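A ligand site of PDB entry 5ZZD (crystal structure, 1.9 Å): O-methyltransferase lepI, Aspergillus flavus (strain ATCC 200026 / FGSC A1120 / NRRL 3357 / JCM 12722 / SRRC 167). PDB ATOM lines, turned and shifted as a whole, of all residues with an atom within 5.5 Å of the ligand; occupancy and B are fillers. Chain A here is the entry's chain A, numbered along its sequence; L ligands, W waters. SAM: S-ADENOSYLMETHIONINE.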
ATOM      1  N   LEU A 193       9.150 -27.429  18.559  1.00  0.00           N
ATOM      2  CA  LEU A 193       9.120 -26.048  17.995  1.00  0.00           C
ATOM      3  C   LEU A 193      10.391 -25.278  18.361  1.00  0.00           C
ATOM      4  O   LEU A 193      10.720 -24.344  17.609  1.00  0.00           O
ATOM      5  CB  LEU A 193       7.902 -25.311  18.553  1.00  0.00           C
ATOM      6  CG  LEU A 193       6.764 -25.061  17.569  1.00  0.00           C
ATOM      7  CD1 LEU A 193       5.969 -23.856  18.053  1.00  0.00           C
ATOM      8  CD2 LEU A 193       7.269 -24.841  16.154  1.00  0.00           C
ATOM      9  N   ASP A 225       5.998 -13.066   9.672  1.00  0.00           N
ATOM     10  CA  ASP A 225       6.380 -14.496   9.818  1.00  0.00           C
ATOM     11  C   ASP A 225       5.124 -15.324  10.086  1.00  0.00           C
ATOM     12  O   ASP A 225       4.684 -15.364  11.259  1.00  0.00           O
ATOM     13  CB  ASP A 225       7.439 -14.634  10.898  1.00  0.00           C
ATOM     14  CG  ASP A 225       8.122 -15.977  10.947  1.00  0.00           C
ATOM     15  OD1 ASP A 225       7.823 -16.823  10.058  1.00  0.00           O
ATOM     16  OD2 ASP A 225       8.913 -16.184  11.905  1.00  0.00           O
ATOM     17  N   ILE A 226       4.510 -15.895   9.032  1.00  0.00           N
ATOM     18  CA  ILE A 226       3.143 -16.477   9.129  1.00  0.00           C
ATOM     19  C   ILE A 226       3.270 -17.933   9.589  1.00  0.00           C
ATOM     20  O   ILE A 226       3.884 -18.745   8.887  1.00  0.00           O
ATOM     21  CB  ILE A 226       2.398 -16.355   7.799  1.00  0.00           C
ATOM     22  CG1 ILE A 226       2.293 -14.880   7.369  1.00  0.00           C
ATOM     23  CG2 ILE A 226       1.041 -17.018   7.912  1.00  0.00           C
ATOM     24  CD1 ILE A 226       1.659 -14.655   6.015  1.00  0.00           C
ATOM     25  N   GLY A 227       2.742 -18.253  10.766  1.00  0.00           N
ATOM     26  CA  GLY A 227       3.017 -19.524  11.452  1.00  0.00           C
ATOM     27  C   GLY A 227       4.466 -19.617  11.869  1.00  0.00           C
ATOM     28  O   GLY A 227       5.055 -20.669  11.673  1.00  0.00           O
ATOM     29  N   GLY A 228       5.013 -18.553  12.461  1.00  0.00           N
ATOM     30  CA  GLY A 228       6.455 -18.430  12.717  1.00  0.00           C
ATOM     31  C   GLY A 228       6.915 -19.198  13.953  1.00  0.00           C
ATOM     32  O   GLY A 228       8.118 -19.211  14.192  1.00  0.00           O
ATOM     33  N   GLY A 229       6.009 -19.878  14.672  1.00  0.00           N
ATOM     34  CA  GLY A 229       6.379 -20.681  15.850  1.00  0.00           C
ATOM     35  C   GLY A 229       7.011 -19.817  16.916  1.00  0.00           C
ATOM     36  O   GLY A 229       6.394 -18.834  17.301  1.00  0.00           O
ATOM     37  N   MET A 230       8.268 -20.114  17.283  1.00  0.00           N
ATOM     38  CA  MET A 230       9.058 -19.374  18.291  1.00  0.00           C
ATOM     39  C   MET A 230       9.589 -18.060  17.685  1.00  0.00           C
ATOM     40  O   MET A 230      10.150 -17.246  18.424  1.00  0.00           O
ATOM     41  CB  MET A 230      10.229 -20.251  18.753  1.00  0.00           C
ATOM     42  CG  MET A 230       9.793 -21.539  19.471  1.00  0.00           C
ATOM     43  SD  MET A 230       8.864 -21.182  20.983  1.00  0.00           S
ATOM     44  CE  MET A 230       7.175 -21.259  20.400  1.00  0.00           C
ATOM     45  N   HIS A 232      12.031 -17.729  15.286  1.00  0.00           N
ATOM     46  CA  HIS A 232      13.468 -17.844  14.928  1.00  0.00           C
ATOM     47  C   HIS A 232      13.759 -17.001  13.682  1.00  0.00           C
ATOM     48  O   HIS A 232      14.820 -16.370  13.646  1.00  0.00           O
ATOM     49  CB  HIS A 232      13.895 -19.301  14.755  1.00  0.00           C
ATOM     50  CG  HIS A 232      13.683 -20.156  15.959  1.00  0.00           C
ATOM     51  ND1 HIS A 232      13.154 -21.432  15.871  1.00  0.00           N
ATOM     52  CD2 HIS A 232      13.964 -19.949  17.272  1.00  0.00           C
ATOM     53  CE1 HIS A 232      13.117 -21.964  17.077  1.00  0.00           C
ATOM     54  NE2 HIS A 232      13.588 -21.071  17.953  1.00  0.00           N
ATOM     55  N   GLN A 251       3.513 -14.086  13.590  1.00  0.00           N
ATOM     56  CA  GLN A 251       2.087 -14.486  13.599  1.00  0.00           C
ATOM     57  C   GLN A 251       1.977 -15.982  13.873  1.00  0.00           C
ATOM     58  O   GLN A 251       2.646 -16.817  13.196  1.00  0.00           O
ATOM     59  CB  GLN A 251       1.398 -14.139  12.275  1.00  0.00           C
ATOM     60  CG  GLN A 251       1.069 -12.653  12.132  1.00  0.00           C
ATOM     61  CD  GLN A 251       0.437 -12.304  10.804  1.00  0.00           C
ATOM     62  OE1 GLN A 251       0.375 -13.134   9.886  1.00  0.00           O
ATOM     63  NE2 GLN A 251      -0.044 -11.069  10.704  1.00  0.00           N
ATOM     64  N   ASP A 252       1.159 -16.353  14.841  1.00  0.00           N
ATOM     65  CA  ASP A 252       0.913 -17.775  15.170  1.00  0.00           C
ATOM     66  C   ASP A 252      -0.343 -17.826  16.047  1.00  0.00           C
ATOM     67  O   ASP A 252      -1.002 -16.764  16.200  1.00  0.00           O
ATOM     68  CB  ASP A 252       2.150 -18.419  15.798  1.00  0.00           C
ATOM     69  CG  ASP A 252       2.295 -19.906  15.478  1.00  0.00           C
ATOM     70  OD1 ASP A 252       1.417 -20.651  15.886  1.00  0.00           O
ATOM     71  OD2 ASP A 252       3.263 -20.276  14.762  1.00  0.00           O
ATOM     72  N   LEU A 253      -0.646 -18.982  16.624  1.00  0.00           N
ATOM     73  CA  LEU A 253      -1.811 -19.144  17.526  1.00  0.00           C
ATOM     74  C   LEU A 253      -1.409 -18.770  18.947  1.00  0.00           C
ATOM     75  O   LEU A 253      -0.246 -18.862  19.319  1.00  0.00           O
ATOM     76  CB  LEU A 253      -2.344 -20.578  17.426  1.00  0.00           C
ATOM     77  CG  LEU A 253      -2.736 -21.033  16.022  1.00  0.00           C
ATOM     78  CD1 LEU A 253      -3.382 -22.403  16.066  1.00  0.00           C
ATOM     79  CD2 LEU A 253      -3.681 -20.039  15.359  1.00  0.00           C
ATOM     80  N   VAL A 256       1.130 -20.706  21.104  1.00  0.00           N
ATOM     81  CA  VAL A 256       2.521 -20.736  20.564  1.00  0.00           C
ATOM     82  C   VAL A 256       3.169 -19.363  20.808  1.00  0.00           C
ATOM     83  O   VAL A 256       4.309 -19.332  21.288  1.00  0.00           O
ATOM     84  CB  VAL A 256       2.521 -21.161  19.081  1.00  0.00           C
ATOM     85  CG1 VAL A 256       3.902 -21.060  18.459  1.00  0.00           C
ATOM     86  CG2 VAL A 256       1.962 -22.569  18.944  1.00  0.00           C
ATOM     87  N   HIS A 274      -2.742 -14.721  14.943  1.00  0.00           N
ATOM     88  CA  HIS A 274      -3.352 -14.794  13.591  1.00  0.00           C
ATOM     89  C   HIS A 274      -3.463 -16.250  13.162  1.00  0.00           C
ATOM     90  O   HIS A 274      -2.460 -16.984  13.241  1.00  0.00           O
ATOM     91  CB  HIS A 274      -2.563 -13.957  12.572  1.00  0.00           C
ATOM     92  CG  HIS A 274      -3.097 -14.106  11.182  1.00  0.00           C
ATOM     93  ND1 HIS A 274      -4.425 -13.855  10.859  1.00  0.00           N
ATOM     94  CD2 HIS A 274      -2.491 -14.515  10.043  1.00  0.00           C
ATOM     95  CE1 HIS A 274      -4.604 -14.102   9.576  1.00  0.00           C
ATOM     96  NE2 HIS A 274      -3.436 -14.483   9.048  1.00  0.00           N
ATOM     97  N   ASN A 275      -4.667 -16.633  12.767  1.00  0.00           N
ATOM     98  CA  ASN A 275      -4.960 -17.946  12.159  1.00  0.00           C
ATOM     99  C   ASN A 275      -4.755 -17.798  10.648  1.00  0.00           C
ATOM    100  O   ASN A 275      -5.410 -16.917  10.051  1.00  0.00           O
ATOM    101  CB  ASN A 275      -6.365 -18.395  12.558  1.00  0.00           C
ATOM    102  CG  ASN A 275      -6.643 -19.806  12.086  1.00  0.00           C
ATOM    103  OD1 ASN A 275      -6.216 -20.178  10.989  1.00  0.00           O
ATOM    104  ND2 ASN A 275      -7.354 -20.577  12.879  1.00  0.00           N
ATOM    105  N   PHE A 276      -3.835 -18.550  10.036  1.00  0.00           N
ATOM    106  CA  PHE A 276      -3.461 -18.324   8.616  1.00  0.00           C
ATOM    107  C   PHE A 276      -4.549 -18.869   7.676  1.00  0.00           C
ATOM    108  O   PHE A 276      -4.452 -18.632   6.430  1.00  0.00           O
ATOM    109  CB  PHE A 276      -2.054 -18.840   8.300  1.00  0.00           C
ATOM    110  CG  PHE A 276      -1.738 -20.284   8.648  1.00  0.00           C
ATOM    111  CD1 PHE A 276      -2.595 -21.321   8.286  1.00  0.00           C
ATOM    112  CD2 PHE A 276      -0.535 -20.593   9.257  1.00  0.00           C
ATOM    113  CE1 PHE A 276      -2.256 -22.636   8.570  1.00  0.00           C
ATOM    114  CE2 PHE A 276      -0.187 -21.917   9.499  1.00  0.00           C
ATOM    115  CZ  PHE A 276      -1.046 -22.935   9.167  1.00  0.00           C
ATOM    116  N   HIS A 277      -5.635 -19.431   8.231  1.00  0.00           N
ATOM    117  CA  HIS A 277      -6.895 -19.747   7.479  1.00  0.00           C
ATOM    118  C   HIS A 277      -7.825 -18.533   7.373  1.00  0.00           C
ATOM    119  O   HIS A 277      -8.872 -18.695   6.750  1.00  0.00           O
ATOM    120  CB  HIS A 277      -7.626 -20.919   8.123  1.00  0.00           C
ATOM    121  CG  HIS A 277      -6.845 -22.192   8.019  1.00  0.00           C
ATOM    122  ND1 HIS A 277      -6.562 -22.754   6.806  1.00  0.00           N
ATOM    123  CD2 HIS A 277      -6.263 -22.963   8.952  1.00  0.00           C
ATOM    124  CE1 HIS A 277      -5.843 -23.840   6.997  1.00  0.00           C
ATOM    125  NE2 HIS A 277      -5.658 -23.985   8.317  1.00  0.00           N
ATOM    126  N   LEU A 290       6.418 -17.803   4.783  1.00  0.00           N
ATOM    127  CA  LEU A 290       5.819 -19.120   5.110  1.00  0.00           C
ATOM    128  C   LEU A 290       6.919 -20.186   5.086  1.00  0.00           C
ATOM    129  O   LEU A 290       7.274 -20.638   3.987  1.00  0.00           O
ATOM    130  CB  LEU A 290       4.749 -19.467   4.083  1.00  0.00           C
ATOM    131  CG  LEU A 290       3.519 -18.566   4.085  1.00  0.00           C
ATOM    132  CD1 LEU A 290       2.753 -18.697   2.779  1.00  0.00           C
ATOM    133  CD2 LEU A 290       2.611 -18.910   5.255  1.00  0.00           C
ATOM    134  N   ARG A 291       7.485 -20.522   6.253  1.00  0.00           N
ATOM    135  CA  ARG A 291       8.567 -21.522   6.351  1.00  0.00           C
ATOM    136  C   ARG A 291       7.990 -22.834   6.900  1.00  0.00           C
ATOM    137  O   ARG A 291       7.494 -22.842   8.064  1.00  0.00           O
ATOM    138  CB  ARG A 291       9.726 -21.047   7.224  1.00  0.00           C
ATOM    139  CG  ARG A 291      10.839 -22.079   7.309  1.00  0.00           C
ATOM    140  CD  ARG A 291      12.165 -21.483   7.709  1.00  0.00           C
ATOM    141  NE  ARG A 291      12.132 -21.155   9.120  1.00  0.00           N
ATOM    142  CZ  ARG A 291      13.003 -20.371   9.733  1.00  0.00           C
ATOM    143  NH1 ARG A 291      14.025 -19.857   9.067  1.00  0.00           N
ATOM    144  NH2 ARG A 291      12.895 -20.161  11.029  1.00  0.00           N
ATOM    145  N   LEU A 292       8.104 -23.891   6.090  1.00  0.00           N
ATOM    146  CA  LEU A 292       7.658 -25.269   6.381  1.00  0.00           C
ATOM    147  C   LEU A 292       6.196 -25.213   6.848  1.00  0.00           C
ATOM    148  O   LEU A 292       5.850 -25.903   7.822  1.00  0.00           O
ATOM    149  CB  LEU A 292       8.571 -25.886   7.442  1.00  0.00           C
ATOM    150  CG  LEU A 292      10.010 -26.185   7.015  1.00  0.00           C
ATOM    151  CD1 LEU A 292      10.802 -26.782   8.165  1.00  0.00           C
ATOM    152  CD2 LEU A 292      10.047 -27.099   5.814  1.00  0.00           C
ATOM    153  N   ILE A 293       5.381 -24.414   6.177  1.00  0.00           N
ATOM    154  CA  ILE A 293       3.931 -24.338   6.448  1.00  0.00           C
ATOM    155  C   ILE A 293       3.208 -25.144   5.363  1.00  0.00           C
ATOM    156  O   ILE A 293       2.447 -26.062   5.708  1.00  0.00           O
ATOM    157  CB  ILE A 293       3.430 -22.874   6.451  1.00  0.00           C
ATOM    158  CG1 ILE A 293       4.159 -22.033   7.509  1.00  0.00           C
ATOM    159  CG2 ILE A 293       1.923 -22.841   6.645  1.00  0.00           C
ATOM    160  CD1 ILE A 293       4.095 -22.612   8.898  1.00  0.00           C
ATOM    161  N   ASP A 296       2.669 -28.990   4.743  1.00  0.00           N
ATOM    162  CA  ASP A 296       1.824 -29.796   5.671  1.00  0.00           C
ATOM    163  C   ASP A 296       0.368 -29.824   5.220  1.00  0.00           C
ATOM    164  O   ASP A 296      -0.478 -30.391   5.968  1.00  0.00           O
ATOM    165  CB  ASP A 296       1.997 -29.276   7.098  1.00  0.00           C
ATOM    166  CG  ASP A 296       3.294 -29.741   7.741  1.00  0.00           C
ATOM    167  OD1 ASP A 296       3.954 -30.619   7.170  1.00  0.00           O
ATOM    168  OD2 ASP A 296       3.626 -29.219   8.802  1.00  0.00           O
ATOM    169  N   PHE A 297       0.068 -29.282   4.043  1.00  0.00           N
ATOM    170  CA  PHE A 297      -1.298 -29.095   3.499  1.00  0.00           C
ATOM    171  C   PHE A 297      -1.355 -29.635   2.078  1.00  0.00           C
ATOM    172  O   PHE A 297      -0.492 -29.334   1.263  1.00  0.00           O
ATOM    173  CB  PHE A 297      -1.722 -27.625   3.570  1.00  0.00           C
ATOM    174  CG  PHE A 297      -1.824 -27.091   4.986  1.00  0.00           C
ATOM    175  CD1 PHE A 297      -2.966 -27.273   5.732  1.00  0.00           C
ATOM    176  CD2 PHE A 297      -0.721 -26.497   5.600  1.00  0.00           C
ATOM    177  CE1 PHE A 297      -3.031 -26.836   7.054  1.00  0.00           C
ATOM    178  CE2 PHE A 297      -0.776 -26.075   6.924  1.00  0.00           C
ATOM    179  CZ  PHE A 297      -1.931 -26.248   7.644  1.00  0.00           C
HETATM  180  N   SAM L   1       7.653 -21.239  10.317  1.00  0.00           N
HETATM  181  CA  SAM L   1       7.979 -22.060  11.510  1.00  0.00           C
HETATM  182  C   SAM L   1       9.495 -22.276  11.545  1.00  0.00           C
HETATM  183  O   SAM L   1      10.072 -22.222  12.643  1.00  0.00           O
HETATM  184  OXT SAM L   1      10.059 -22.473  10.457  1.00  0.00           O
HETATM  185  CB  SAM L   1       7.234 -23.408  11.414  1.00  0.00           C
HETATM  186  CG  SAM L   1       6.850 -23.961  12.749  1.00  0.00           C
HETATM  187  SD  SAM L   1       5.769 -25.413  12.657  1.00  0.00           S
HETATM  188  CE  SAM L   1       6.495 -26.445  11.371  1.00  0.00           C
HETATM  189  C5' SAM L   1       4.257 -24.751  11.915  1.00  0.00           C
HETATM  190  C4' SAM L   1       3.697 -23.598  12.729  1.00  0.00           C
HETATM  191  O4' SAM L   1       2.367 -23.305  12.257  1.00  0.00           O
HETATM  192  C3' SAM L   1       3.566 -23.859  14.238  1.00  0.00           C
HETATM  193  O3' SAM L   1       4.277 -22.872  14.967  1.00  0.00           O
HETATM  194  C2' SAM L   1       2.057 -23.853  14.482  1.00  0.00           C
HETATM  195  O2' SAM L   1       1.671 -23.290  15.722  1.00  0.00           O
HETATM  196  C1' SAM L   1       1.593 -22.949  13.358  1.00  0.00           C
HETATM  197  N9  SAM L   1       0.193 -23.072  12.989  1.00  0.00           N
HETATM  198  C8  SAM L   1      -0.551 -24.211  12.772  1.00  0.00           C
HETATM  199  N7  SAM L   1      -1.788 -23.965  12.402  1.00  0.00           N
HETATM  200  C5  SAM L   1      -1.852 -22.585  12.338  1.00  0.00           C
HETATM  201  C6  SAM L   1      -2.894 -21.694  11.991  1.00  0.00           C
HETATM  202  N6  SAM L   1      -4.104 -22.096  11.593  1.00  0.00           N
HETATM  203  N1  SAM L   1      -2.601 -20.374  11.977  1.00  0.00           N
HETATM  204  C2  SAM L   1      -1.377 -19.983  12.342  1.00  0.00           C
HETATM  205  N3  SAM L   1      -0.340 -20.708  12.743  1.00  0.00           N
HETATM  206  C4  SAM L   1      -0.633 -22.019  12.690  1.00  0.00           C
HETATM  207  O   HOH W   1       1.316 -25.184  10.056  1.00  0.00           O
HETATM  208  O   HOH W   2      -2.628 -26.351  11.350  1.00  0.00           O
HETATM  209  O   HOH W   3      12.417 -22.606  13.478  1.00  0.00           O
HETATM  210  O   HOH W   4      12.060 -24.406  10.256  1.00  0.00           O
HETATM  211  O   HOH W   5       6.514 -19.152   8.722  1.00  0.00           O
HETATM  212  O   HOH W   6       9.447 -19.093  10.193  1.00  0.00           O
HETATM  213  O   HOH W   7      -5.614 -24.406  12.268  1.00  0.00           O
HETATM  214  O   HOH W   8      -0.396 -24.569  16.987  1.00  0.00           O
HETATM  215  O   HOH W   9       3.438 -26.559   9.194  1.00  0.00           O
HETATM  216  O   HOH W  10       9.613 -22.494  15.856  1.00  0.00           O
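An oxygen (O2') of the ligand is in hydrogen-bond range of the side-chain carboxylate of Asp 252 (2.7 Å). O of Arg 291 lies within hydrogen-bond range of N of the ligand (2.8 Å). NE of Arg 291 lies within salt-bridge range of OXT of the ligand (2.8 Å). The side-chain amide oxygen (OD1) of Asn 275 lies within hydrogen-bond range of a nitrogen (N6) of the ligand (2.9 Å). The backbone NH of Phe 276 lies within hydrogen-bond range of a nitrogen (N1) of the ligand, 2.9 Å away. The backbone carbonyl oxygen (O) of Gly 227 is in hydrogen-bond range of a nitrogen (N) of the ligand (3.0 Å). The backbone NH (N) of Gly 229 lies close to an oxygen (O3') of the ligand (3.5 Å).
Water W3 lies within hydrogen-bond range of an oxygen (O) of the ligand (2.5 Å), a ring nitrogen (ND1) of His 232 (2.8 Å) and the guanidinium group (NH2) of Arg 291 (3.5 Å). Water W4 bridges OXT of the ligand and NE of Arg 291. Water W6 bridges the side-chain carboxylate (OD1) of Asp 225 (2.8 Å) and a nitrogen (N) of the ligand (2.8 Å). Water W5 lies within hydrogen-bond range of O of Ile 226 (2.7 Å), N of the ligand (2.9 Å), N of Arg 291 (3.0 Å) and OD1 of Asp 225 (3.0 Å). Water W10 lies within hydrogen-bond range of O of Leu 193 (2.8 Å), N of Met 230 (3.1 Å) and O of the ligand (3.3 Å). Water W9 bridges OD2 of Asp 296 (2.7 Å) and O of Leu 292 (2.9 Å).
The side-chain carboxylate of Asp 252 lies within hydrogen-bond range of the backbone NH of Gly 229. The backbone carbonyl oxygen of Asp 252 sits at hydrogen-bond distance from the backbone NH of His 274, at 3.0 Å. N of Gly 228 lies within hydrogen-bond range of OD2 of Asp 252. The side-chain amide oxygen of Asn 275 is in hydrogen-bond range of the backbone NH of His 277 (2.9 Å). O of Gln 251 sits at hydrogen-bond distance from N of Gly 227 (2.8 Å). The backbone carbonyl oxygen of Gln 251 lies within hydrogen-bond range of the backbone NH of Gly 228 (3.0 Å).
Merely in contact with the ligand: His 274 (3.3 Å), Val 256 (3.3 Å), His 277 (3.5 Å), Leu 193 (3.5 Å), Leu 253 (3.6 Å), Leu 292 (3.6 Å), Ile 293 (3.7 Å) and Gly 228 (3.9 Å). Hydrophobic or aromatic side chains that line the ligand: Leu 193, Leu 253, Val 256, Phe 276, His 277 and Ile 293. Within 4 Å of the ligand: Leu 193, Gly 227, Gly 228, Gly 229, Asp 252, Leu 253, Val 256, His 274, Asn 275, Phe 276, His 277, Arg 291, Leu 292 and Ile 293. Along chain A the residues within 4 Å of the ligand span positions 193 to 293. The nearest printed residue that does not touch the ligand is Asp 225 (4.4 Å).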
